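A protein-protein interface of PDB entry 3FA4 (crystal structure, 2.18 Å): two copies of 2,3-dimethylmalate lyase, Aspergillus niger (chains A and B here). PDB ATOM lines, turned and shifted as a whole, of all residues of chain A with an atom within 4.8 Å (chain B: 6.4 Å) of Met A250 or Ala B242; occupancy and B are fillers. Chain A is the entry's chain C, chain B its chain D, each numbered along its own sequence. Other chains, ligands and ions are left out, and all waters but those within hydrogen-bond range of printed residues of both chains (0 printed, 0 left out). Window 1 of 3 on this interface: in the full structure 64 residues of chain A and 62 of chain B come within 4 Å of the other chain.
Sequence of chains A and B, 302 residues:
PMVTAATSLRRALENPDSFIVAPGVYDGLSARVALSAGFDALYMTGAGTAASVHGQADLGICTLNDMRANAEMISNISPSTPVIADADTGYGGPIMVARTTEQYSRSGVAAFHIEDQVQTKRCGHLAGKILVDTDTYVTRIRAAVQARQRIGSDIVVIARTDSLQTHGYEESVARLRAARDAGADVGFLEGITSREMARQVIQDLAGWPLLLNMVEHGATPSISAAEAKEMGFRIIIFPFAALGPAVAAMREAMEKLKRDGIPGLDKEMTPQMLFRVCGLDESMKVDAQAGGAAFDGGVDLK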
ATOM      1  N   ALA A 246      -8.989  -9.969  -6.536  1.00  0.00           N
ATOM      2  CA  ALA A 246      -8.316 -10.985  -7.318  1.00  0.00           C
ATOM      3  C   ALA A 246      -7.737 -10.339  -8.543  1.00  0.00           C
ATOM      4  O   ALA A 246      -6.636 -10.605  -8.842  1.00  0.00           O
ATOM      5  CB  ALA A 246      -9.212 -12.170  -7.673  1.00  0.00           C
ATOM      6  N   VAL A 247      -8.471  -9.454  -9.218  1.00  0.00           N
ATOM      7  CA  VAL A 247      -8.037  -8.889 -10.537  1.00  0.00           C
ATOM      8  C   VAL A 247      -6.806  -8.022 -10.339  1.00  0.00           C
ATOM      9  O   VAL A 247      -5.792  -8.277 -10.958  1.00  0.00           O
ATOM     10  CB  VAL A 247      -9.190  -8.101 -11.233  1.00  0.00           C
ATOM     11  CG1 VAL A 247      -8.706  -7.377 -12.474  1.00  0.00           C
ATOM     12  CG2 VAL A 247     -10.403  -9.044 -11.587  1.00  0.00           C
ATOM     13  N   ALA A 248      -6.887  -7.010  -9.442  1.00  0.00           N
ATOM     14  CA  ALA A 248      -5.724  -6.117  -9.112  1.00  0.00           C
ATOM     15  C   ALA A 248      -4.477  -6.921  -8.726  1.00  0.00           C
ATOM     16  O   ALA A 248      -3.416  -6.665  -9.225  1.00  0.00           O
ATOM     17  CB  ALA A 248      -6.091  -5.094  -8.013  1.00  0.00           C
ATOM     18  N   ALA A 249      -4.599  -7.950  -7.896  1.00  0.00           N
ATOM     19  CA  ALA A 249      -3.392  -8.749  -7.581  1.00  0.00           C
ATOM     20  C   ALA A 249      -2.834  -9.639  -8.713  1.00  0.00           C
ATOM     21  O   ALA A 249      -1.653  -9.730  -8.872  1.00  0.00           O
ATOM     22  CB  ALA A 249      -3.592  -9.533  -6.342  1.00  0.00           C
ATOM     23  N   MET A 250      -3.675 -10.280  -9.505  1.00  0.00           N
ATOM     24  CA  MET A 250      -3.187 -11.045 -10.659  1.00  0.00           C
ATOM     25  C   MET A 250      -2.596 -10.120 -11.692  1.00  0.00           C
ATOM     26  O   MET A 250      -1.598 -10.450 -12.298  1.00  0.00           O
ATOM     27  CB  MET A 250      -4.290 -11.871 -11.295  1.00  0.00           C
ATOM     28  CG  MET A 250      -4.864 -12.997 -10.482  1.00  0.00           C
ATOM     29  SD  MET A 250      -6.047 -13.975 -11.402  1.00  0.00           S
ATOM     30  CE  MET A 250      -7.545 -12.940 -11.348  1.00  0.00           C
ATOM     31  N   ARG A 251      -3.182  -8.944 -11.917  1.00  0.00           N
ATOM     32  CA  ARG A 251      -2.575  -8.019 -12.919  1.00  0.00           C
ATOM     33  C   ARG A 251      -1.147  -7.588 -12.520  1.00  0.00           C
ATOM     34  O   ARG A 251      -0.197  -7.691 -13.326  1.00  0.00           O
ATOM     35  CB  ARG A 251      -3.485  -6.807 -13.232  1.00  0.00           C
ATOM     36  CG  ARG A 251      -2.696  -5.571 -13.603  1.00  0.00           C
ATOM     37  CD  ARG A 251      -3.467  -4.257 -13.866  1.00  0.00           C
ATOM     38  NE  ARG A 251      -4.876  -4.306 -13.506  1.00  0.00           N
ATOM     39  CZ  ARG A 251      -5.411  -3.665 -12.456  1.00  0.00           C
ATOM     40  NH1 ARG A 251      -4.627  -2.898 -11.658  1.00  0.00           N
ATOM     41  NH2 ARG A 251      -6.744  -3.809 -12.218  1.00  0.00           N
ATOM     42  N   GLU A 252      -0.982  -7.150 -11.268  1.00  0.00           N
ATOM     43  CA  GLU A 252       0.352  -6.899 -10.707  1.00  0.00           C
ATOM     44  C   GLU A 252       1.363  -8.064 -10.749  1.00  0.00           C
ATOM     45  O   GLU A 252       2.554  -7.862 -11.077  1.00  0.00           O
ATOM     46  CB  GLU A 252       0.212  -6.338  -9.303  1.00  0.00           C
ATOM     47  CG  GLU A 252      -0.643  -5.082  -9.311  1.00  0.00           C
ATOM     48  CD  GLU A 252      -0.801  -4.483  -7.921  1.00  0.00           C
ATOM     49  OE1 GLU A 252      -0.139  -5.018  -6.973  1.00  0.00           O
ATOM     50  OE2 GLU A 252      -1.562  -3.473  -7.766  1.00  0.00           O
ATOM     51  N   ALA A 253       0.887  -9.277 -10.438  1.00  0.00           N
ATOM     52  CA  ALA A 253       1.703 -10.511 -10.493  1.00  0.00           C
ATOM     53  C   ALA A 253       2.187 -10.765 -11.877  1.00  0.00           C
ATOM     54  O   ALA A 253       3.353 -10.973 -12.077  1.00  0.00           O
ATOM     55  CB  ALA A 253       0.908 -11.676 -10.020  1.00  0.00           C
ATOM     56  N   MET A 254       1.273 -10.738 -12.842  1.00  0.00           N
ATOM     57  CA  MET A 254       1.593 -10.892 -14.273  1.00  0.00           C
ATOM     58  C   MET A 254       2.524  -9.830 -14.817  1.00  0.00           C
ATOM     59  O   MET A 254       3.422 -10.153 -15.558  1.00  0.00           O
ATOM     60  CB  MET A 254       0.320 -10.908 -15.089  1.00  0.00           C
ATOM     61  CG  MET A 254      -0.506 -12.109 -14.838  1.00  0.00           C
ATOM     62  SD  MET A 254       0.204 -13.690 -15.356  1.00  0.00           S
ATOM     63  CE  MET A 254      -1.101 -14.762 -14.711  1.00  0.00           C
ATOM     64  N   PRO B  23       2.449 -18.237 -18.594  1.00  0.00           N
ATOM     65  CA  PRO B  23       1.898 -18.334 -17.216  1.00  0.00           C
ATOM     66  C   PRO B  23       0.687 -19.197 -17.103  1.00  0.00           C
ATOM     67  O   PRO B  23      -0.176 -19.255 -18.007  1.00  0.00           O
ATOM     68  CB  PRO B  23       1.407 -16.881 -16.935  1.00  0.00           C
ATOM     69  CG  PRO B  23       1.996 -16.097 -17.895  1.00  0.00           C
ATOM     70  CD  PRO B  23       2.154 -16.904 -19.158  1.00  0.00           C
ATOM     71  N   GLY B  24       0.509 -19.748 -15.934  1.00  0.00           N
ATOM     72  CA  GLY B  24      -0.687 -20.434 -15.631  1.00  0.00           C
ATOM     73  C   GLY B  24      -1.905 -19.623 -15.299  1.00  0.00           C
ATOM     74  O   GLY B  24      -1.950 -18.758 -14.391  1.00  0.00           O
ATOM     75  N   VAL B  25      -2.963 -20.039 -15.996  1.00  0.00           N
ATOM     76  CA  VAL B  25      -4.233 -19.404 -15.969  1.00  0.00           C
ATOM     77  C   VAL B  25      -5.169 -20.535 -15.770  1.00  0.00           C
ATOM     78  O   VAL B  25      -4.889 -21.671 -16.190  1.00  0.00           O
ATOM     79  CB  VAL B  25      -4.531 -18.586 -17.275  1.00  0.00           C
ATOM     80  CG1 VAL B  25      -3.642 -17.314 -17.340  1.00  0.00           C
ATOM     81  CG2 VAL B  25      -4.465 -19.461 -18.493  1.00  0.00           C
ATOM     82  N   TYR B  26      -6.251 -20.255 -15.041  1.00  0.00           N
ATOM     83  CA  TYR B  26      -7.175 -21.245 -14.639  1.00  0.00           C
ATOM     84  C   TYR B  26      -8.599 -20.958 -15.051  1.00  0.00           C
ATOM     85  O   TYR B  26      -9.441 -21.829 -14.905  1.00  0.00           O
ATOM     86  CB  TYR B  26      -7.075 -21.412 -13.118  1.00  0.00           C
ATOM     87  CG  TYR B  26      -7.400 -20.237 -12.209  1.00  0.00           C
ATOM     88  CD1 TYR B  26      -6.426 -19.311 -11.845  1.00  0.00           C
ATOM     89  CD2 TYR B  26      -8.668 -20.086 -11.687  1.00  0.00           C
ATOM     90  CE1 TYR B  26      -6.707 -18.250 -10.979  1.00  0.00           C
ATOM     91  CE2 TYR B  26      -9.023 -19.012 -10.820  1.00  0.00           C
ATOM     92  CZ  TYR B  26      -8.039 -18.118 -10.464  1.00  0.00           C
ATOM     93  OH  TYR B  26      -8.347 -17.094  -9.627  1.00  0.00           O
ATOM     94  N   ASP B  27      -8.892 -19.734 -15.534  1.00  0.00           N
ATOM     95  CA  ASP B  27     -10.269 -19.230 -15.764  1.00  0.00           C
ATOM     96  C   ASP B  27     -10.243 -18.074 -16.699  1.00  0.00           C
ATOM     97  O   ASP B  27      -9.189 -17.677 -17.140  1.00  0.00           O
ATOM     98  CB  ASP B  27     -11.085 -18.944 -14.470  1.00  0.00           C
ATOM     99  CG  ASP B  27     -10.743 -17.614 -13.758  1.00  0.00           C
ATOM    100  OD1 ASP B  27      -9.716 -16.992 -14.052  1.00  0.00           O
ATOM    101  OD2 ASP B  27     -11.481 -17.227 -12.847  1.00  0.00           O
ATOM    102  N   LEU B  29     -10.882 -14.844 -16.276  1.00  0.00           N
ATOM    103  CA  LEU B  29     -10.258 -13.661 -15.677  1.00  0.00           C
ATOM    104  C   LEU B  29      -8.752 -13.709 -15.689  1.00  0.00           C
ATOM    105  O   LEU B  29      -8.131 -12.739 -15.972  1.00  0.00           O
ATOM    106  CB  LEU B  29     -10.618 -13.514 -14.203  1.00  0.00           C
ATOM    107  CG  LEU B  29     -11.680 -12.506 -13.894  1.00  0.00           C
ATOM    108  CD1 LEU B  29     -11.944 -12.333 -12.360  1.00  0.00           C
ATOM    109  CD2 LEU B  29     -11.340 -11.210 -14.501  1.00  0.00           C
ATOM    110  N   SER B  30      -8.192 -14.846 -15.288  1.00  0.00           N
ATOM    111  CA  SER B  30      -6.791 -14.876 -15.089  1.00  0.00           C
ATOM    112  C   SER B  30      -6.194 -14.946 -16.472  1.00  0.00           C
ATOM    113  O   SER B  30      -5.089 -14.529 -16.658  1.00  0.00           O
ATOM    114  CB  SER B  30      -6.410 -16.035 -14.195  1.00  0.00           C
ATOM    115  OG  SER B  30      -7.040 -17.198 -14.685  1.00  0.00           O
ATOM    116  N   ALA B  31      -6.959 -15.388 -17.475  1.00  0.00           N
ATOM    117  CA  ALA B  31      -6.462 -15.399 -18.841  1.00  0.00           C
ATOM    118  C   ALA B  31      -6.532 -14.021 -19.509  1.00  0.00           C
ATOM    119  O   ALA B  31      -5.689 -13.731 -20.355  1.00  0.00           O
ATOM    120  CB  ALA B  31      -7.157 -16.437 -19.670  1.00  0.00           C
ATOM    121  N   VAL B  33      -6.231 -11.199 -17.866  1.00  0.00           N
ATOM    122  CA  VAL B  33      -5.218 -10.493 -17.131  1.00  0.00           C
ATOM    123  C   VAL B  33      -3.798 -10.788 -17.575  1.00  0.00           C
ATOM    124  O   VAL B  33      -3.039  -9.864 -17.648  1.00  0.00           O
ATOM    125  CB  VAL B  33      -5.398 -10.691 -15.601  1.00  0.00           C
ATOM    126  CG1 VAL B  33      -4.237 -10.073 -14.837  1.00  0.00           C
ATOM    127  CG2 VAL B  33      -6.705 -10.003 -15.118  1.00  0.00           C
ATOM    128  N   ALA B  34      -3.468 -12.054 -17.910  1.00  0.00           N
ATOM    129  CA  ALA B  34      -2.158 -12.449 -18.483  1.00  0.00           C
ATOM    130  C   ALA B  34      -1.937 -11.962 -19.913  1.00  0.00           C
ATOM    131  O   ALA B  34      -0.908 -11.500 -20.231  1.00  0.00           O
ATOM    132  CB  ALA B  34      -2.015 -13.993 -18.440  1.00  0.00           C
ATOM    133  N   PHE B 238       4.429 -21.615 -15.681  1.00  0.00           N
ATOM    134  CA  PHE B 238       4.355 -20.987 -14.368  1.00  0.00           C
ATOM    135  C   PHE B 238       2.962 -21.220 -13.867  1.00  0.00           C
ATOM    136  O   PHE B 238       2.184 -20.229 -13.707  1.00  0.00           O
ATOM    137  CB  PHE B 238       4.636 -19.461 -14.366  1.00  0.00           C
ATOM    138  CG  PHE B 238       5.997 -19.078 -14.841  1.00  0.00           C
ATOM    139  CD1 PHE B 238       6.181 -18.590 -16.159  1.00  0.00           C
ATOM    140  CD2 PHE B 238       7.103 -19.186 -14.006  1.00  0.00           C
ATOM    141  CE1 PHE B 238       7.430 -18.234 -16.598  1.00  0.00           C
ATOM    142  CE2 PHE B 238       8.366 -18.846 -14.459  1.00  0.00           C
ATOM    143  CZ  PHE B 238       8.524 -18.359 -15.755  1.00  0.00           C
ATOM    144  N   PRO B 239       2.656 -22.488 -13.527  1.00  0.00           N
ATOM    145  CA  PRO B 239       1.287 -22.856 -13.134  1.00  0.00           C
ATOM    146  C   PRO B 239       0.634 -21.998 -12.085  1.00  0.00           C
ATOM    147  O   PRO B 239      -0.578 -21.844 -12.163  1.00  0.00           O
ATOM    148  CB  PRO B 239       1.396 -24.313 -12.683  1.00  0.00           C
ATOM    149  CG  PRO B 239       2.616 -24.830 -13.478  1.00  0.00           C
ATOM    150  CD  PRO B 239       3.565 -23.660 -13.471  1.00  0.00           C
ATOM    151  N   PHE B 240       1.413 -21.403 -11.168  1.00  0.00           N
ATOM    152  CA  PHE B 240       0.884 -20.787  -9.945  1.00  0.00           C
ATOM    153  C   PHE B 240       0.935 -19.237 -10.020  1.00  0.00           C
ATOM    154  O   PHE B 240       0.551 -18.549  -9.046  1.00  0.00           O
ATOM    155  CB  PHE B 240       1.622 -21.334  -8.694  1.00  0.00           C
ATOM    156  CG  PHE B 240       0.678 -21.736  -7.528  1.00  0.00           C
ATOM    157  CD1 PHE B 240       0.498 -20.905  -6.440  1.00  0.00           C
ATOM    158  CD2 PHE B 240      -0.033 -22.941  -7.576  1.00  0.00           C
ATOM    159  CE1 PHE B 240      -0.426 -21.247  -5.413  1.00  0.00           C
ATOM    160  CE2 PHE B 240      -0.910 -23.299  -6.589  1.00  0.00           C
ATOM    161  CZ  PHE B 240      -1.114 -22.431  -5.497  1.00  0.00           C
ATOM    162  N   ALA B 241       1.379 -18.708 -11.176  1.00  0.00           N
ATOM    163  CA  ALA B 241       1.408 -17.247 -11.480  1.00  0.00           C
ATOM    164  C   ALA B 241       0.174 -16.413 -11.061  1.00  0.00           C
ATOM    165  O   ALA B 241       0.291 -15.259 -10.648  1.00  0.00           O
ATOM    166  CB  ALA B 241       1.670 -17.028 -12.945  1.00  0.00           C
ATOM    167  N   ALA B 242      -1.015 -16.982 -11.210  1.00  0.00           N
ATOM    168  CA  ALA B 242      -2.241 -16.243 -10.978  1.00  0.00           C
ATOM    169  C   ALA B 242      -2.911 -16.753  -9.707  1.00  0.00           C
ATOM    170  O   ALA B 242      -3.530 -15.978  -8.958  1.00  0.00           O
ATOM    171  CB  ALA B 242      -3.107 -16.429 -12.189  1.00  0.00           C
ATOM    172  N   LEU B 243      -2.714 -18.047  -9.405  1.00  0.00           N
ATOM    173  CA  LEU B 243      -3.377 -18.695  -8.272  1.00  0.00           C
ATOM    174  C   LEU B 243      -2.885 -18.091  -6.948  1.00  0.00           C
ATOM    175  O   LEU B 243      -3.716 -17.721  -6.110  1.00  0.00           O
ATOM    176  CB  LEU B 243      -3.198 -20.202  -8.305  1.00  0.00           C
ATOM    177  CG  LEU B 243      -3.991 -21.050  -9.313  1.00  0.00           C
ATOM    178  CD1 LEU B 243      -3.469 -22.463  -9.438  1.00  0.00           C
ATOM    179  CD2 LEU B 243      -5.421 -21.111  -8.830  1.00  0.00           C
ATOM    180  N   GLY B 244      -1.562 -18.027  -6.762  1.00  0.00           N
ATOM    181  CA  GLY B 244      -0.949 -17.501  -5.557  1.00  0.00           C
ATOM    182  C   GLY B 244      -1.469 -16.128  -5.190  1.00  0.00           C
ATOM    183  O   GLY B 244      -2.080 -15.964  -4.141  1.00  0.00           O
ATOM    184  N   PRO B 245      -1.193 -15.123  -6.037  1.00  0.00           N
ATOM    185  CA  PRO B 245      -1.770 -13.757  -5.907  1.00  0.00           C
ATOM    186  C   PRO B 245      -3.302 -13.671  -5.674  1.00  0.00           C
ATOM    187  O   PRO B 245      -3.719 -13.010  -4.694  1.00  0.00           O
ATOM    188  CB  PRO B 245      -1.321 -13.066  -7.212  1.00  0.00           C
ATOM    189  CG  PRO B 245      -0.020 -13.750  -7.502  1.00  0.00           C
ATOM    190  CD  PRO B 245      -0.220 -15.191  -7.152  1.00  0.00           C
ATOM    191  N   ALA B 246      -4.110 -14.365  -6.505  1.00  0.00           N
ATOM    192  CA  ALA B 246      -5.555 -14.424  -6.322  1.00  0.00           C
ATOM    193  C   ALA B 246      -5.933 -14.844  -4.921  1.00  0.00           C
ATOM    194  O   ALA B 246      -6.601 -14.065  -4.234  1.00  0.00           O
ATOM    195  CB  ALA B 246      -6.243 -15.337  -7.378  1.00  0.00           C
ATOM    196  N   VAL B 247      -5.493 -16.038  -4.481  1.00  0.00           N
ATOM    197  CA  VAL B 247      -5.876 -16.560  -3.152  1.00  0.00           C
ATOM    198  C   VAL B 247      -5.508 -15.668  -1.965  1.00  0.00           C
ATOM    199  O   VAL B 247      -6.344 -15.447  -1.086  1.00  0.00           O
ATOM    200  CB  VAL B 247      -5.343 -17.977  -2.888  1.00  0.00           C
ATOM    201  CG1 VAL B 247      -6.032 -18.535  -1.653  1.00  0.00           C
ATOM    202  CG2 VAL B 247      -5.614 -18.873  -4.018  1.00  0.00           C
ATOM    203  N   ALA B 249      -4.711 -12.273  -1.939  1.00  0.00           N
ATOM    204  CA  ALA B 249      -5.566 -11.059  -2.129  1.00  0.00           C
ATOM    205  C   ALA B 249      -7.069 -11.194  -1.648  1.00  0.00           C
ATOM    206  O   ALA B 249      -7.568 -10.413  -0.787  1.00  0.00           O
ATOM    207  CB  ALA B 249      -5.487 -10.626  -3.600  1.00  0.00           C
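The backbone NH of Tyr B26 lies within hydrogen-bond range of the side-chain hydroxyl of Ser B30, at 3.2 Å. The side-chain carboxylate (OD1) of Asp B27 is in hydrogen-bond range of the backbone NH (N) of Leu B29, at 3.3 Å. The side-chain carboxylate of Asp B27 lies within hydrogen-bond range of the side-chain hydroxyl of Ser B30, 2.8 Å away.
Among the printed residues, merely in contact across the chains: Arg A251 with Val B33, Ala A253 with Pro B245, Met A250 with Ser B30, Ala A249 with Ala B249, Met A250 with Val B33, Met A250 with Ala B242, Met A254 with Ala B242, Ala A253 with Ala B241, Val A247 with Leu B29, Ala A249 with Pro B245, Met A254 with Pro B23, Met A254 with Ala B34 and Met A254 with Ala B241.
Of the printed residues of chain B, Val A247 touches Leu B29. Met A250 touches just these residues of chain B: Ser B30 (3.5 Å), Val B33 (3.5 Å) and Ala B242 (3.6 Å). Glu A252 touches none of the printed residues of chain B. Of the printed residues of chain B, Met A254 touches Pro B23, Ala B34, Ala B241 and Ala B242. Of the printed residues of chain A, Leu B29 touches Val A247. Printed residues of chain A within 4 Å of Ser B30: Met A250. Ala B242 touches two residues of chain A. Leu B243 touches none of the printed residues of chain A. Printed residues of chain A within 4 Å of Pro B245: Ala A249 and Ala A253. The nearest residue of chain B that does not touch Met A250 is Ala B246 (4.1 Å).
Printed residues of chain B that touch a printed residue of chain A: Pro B23, Leu B29, Ser B30, Val B33, Ala B34, Ala B241, Ala B242, Pro B245 and Ala B249. Of the 9 printed residues of chain A, 6 touch a printed residue of chain B. Among the printed residues, no Asp or Glu carboxylate lies within 4 Å of a Lys or Arg side-chain nitrogen of the other chain.
Ala B249 touches its own counterpart, Ala A249.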
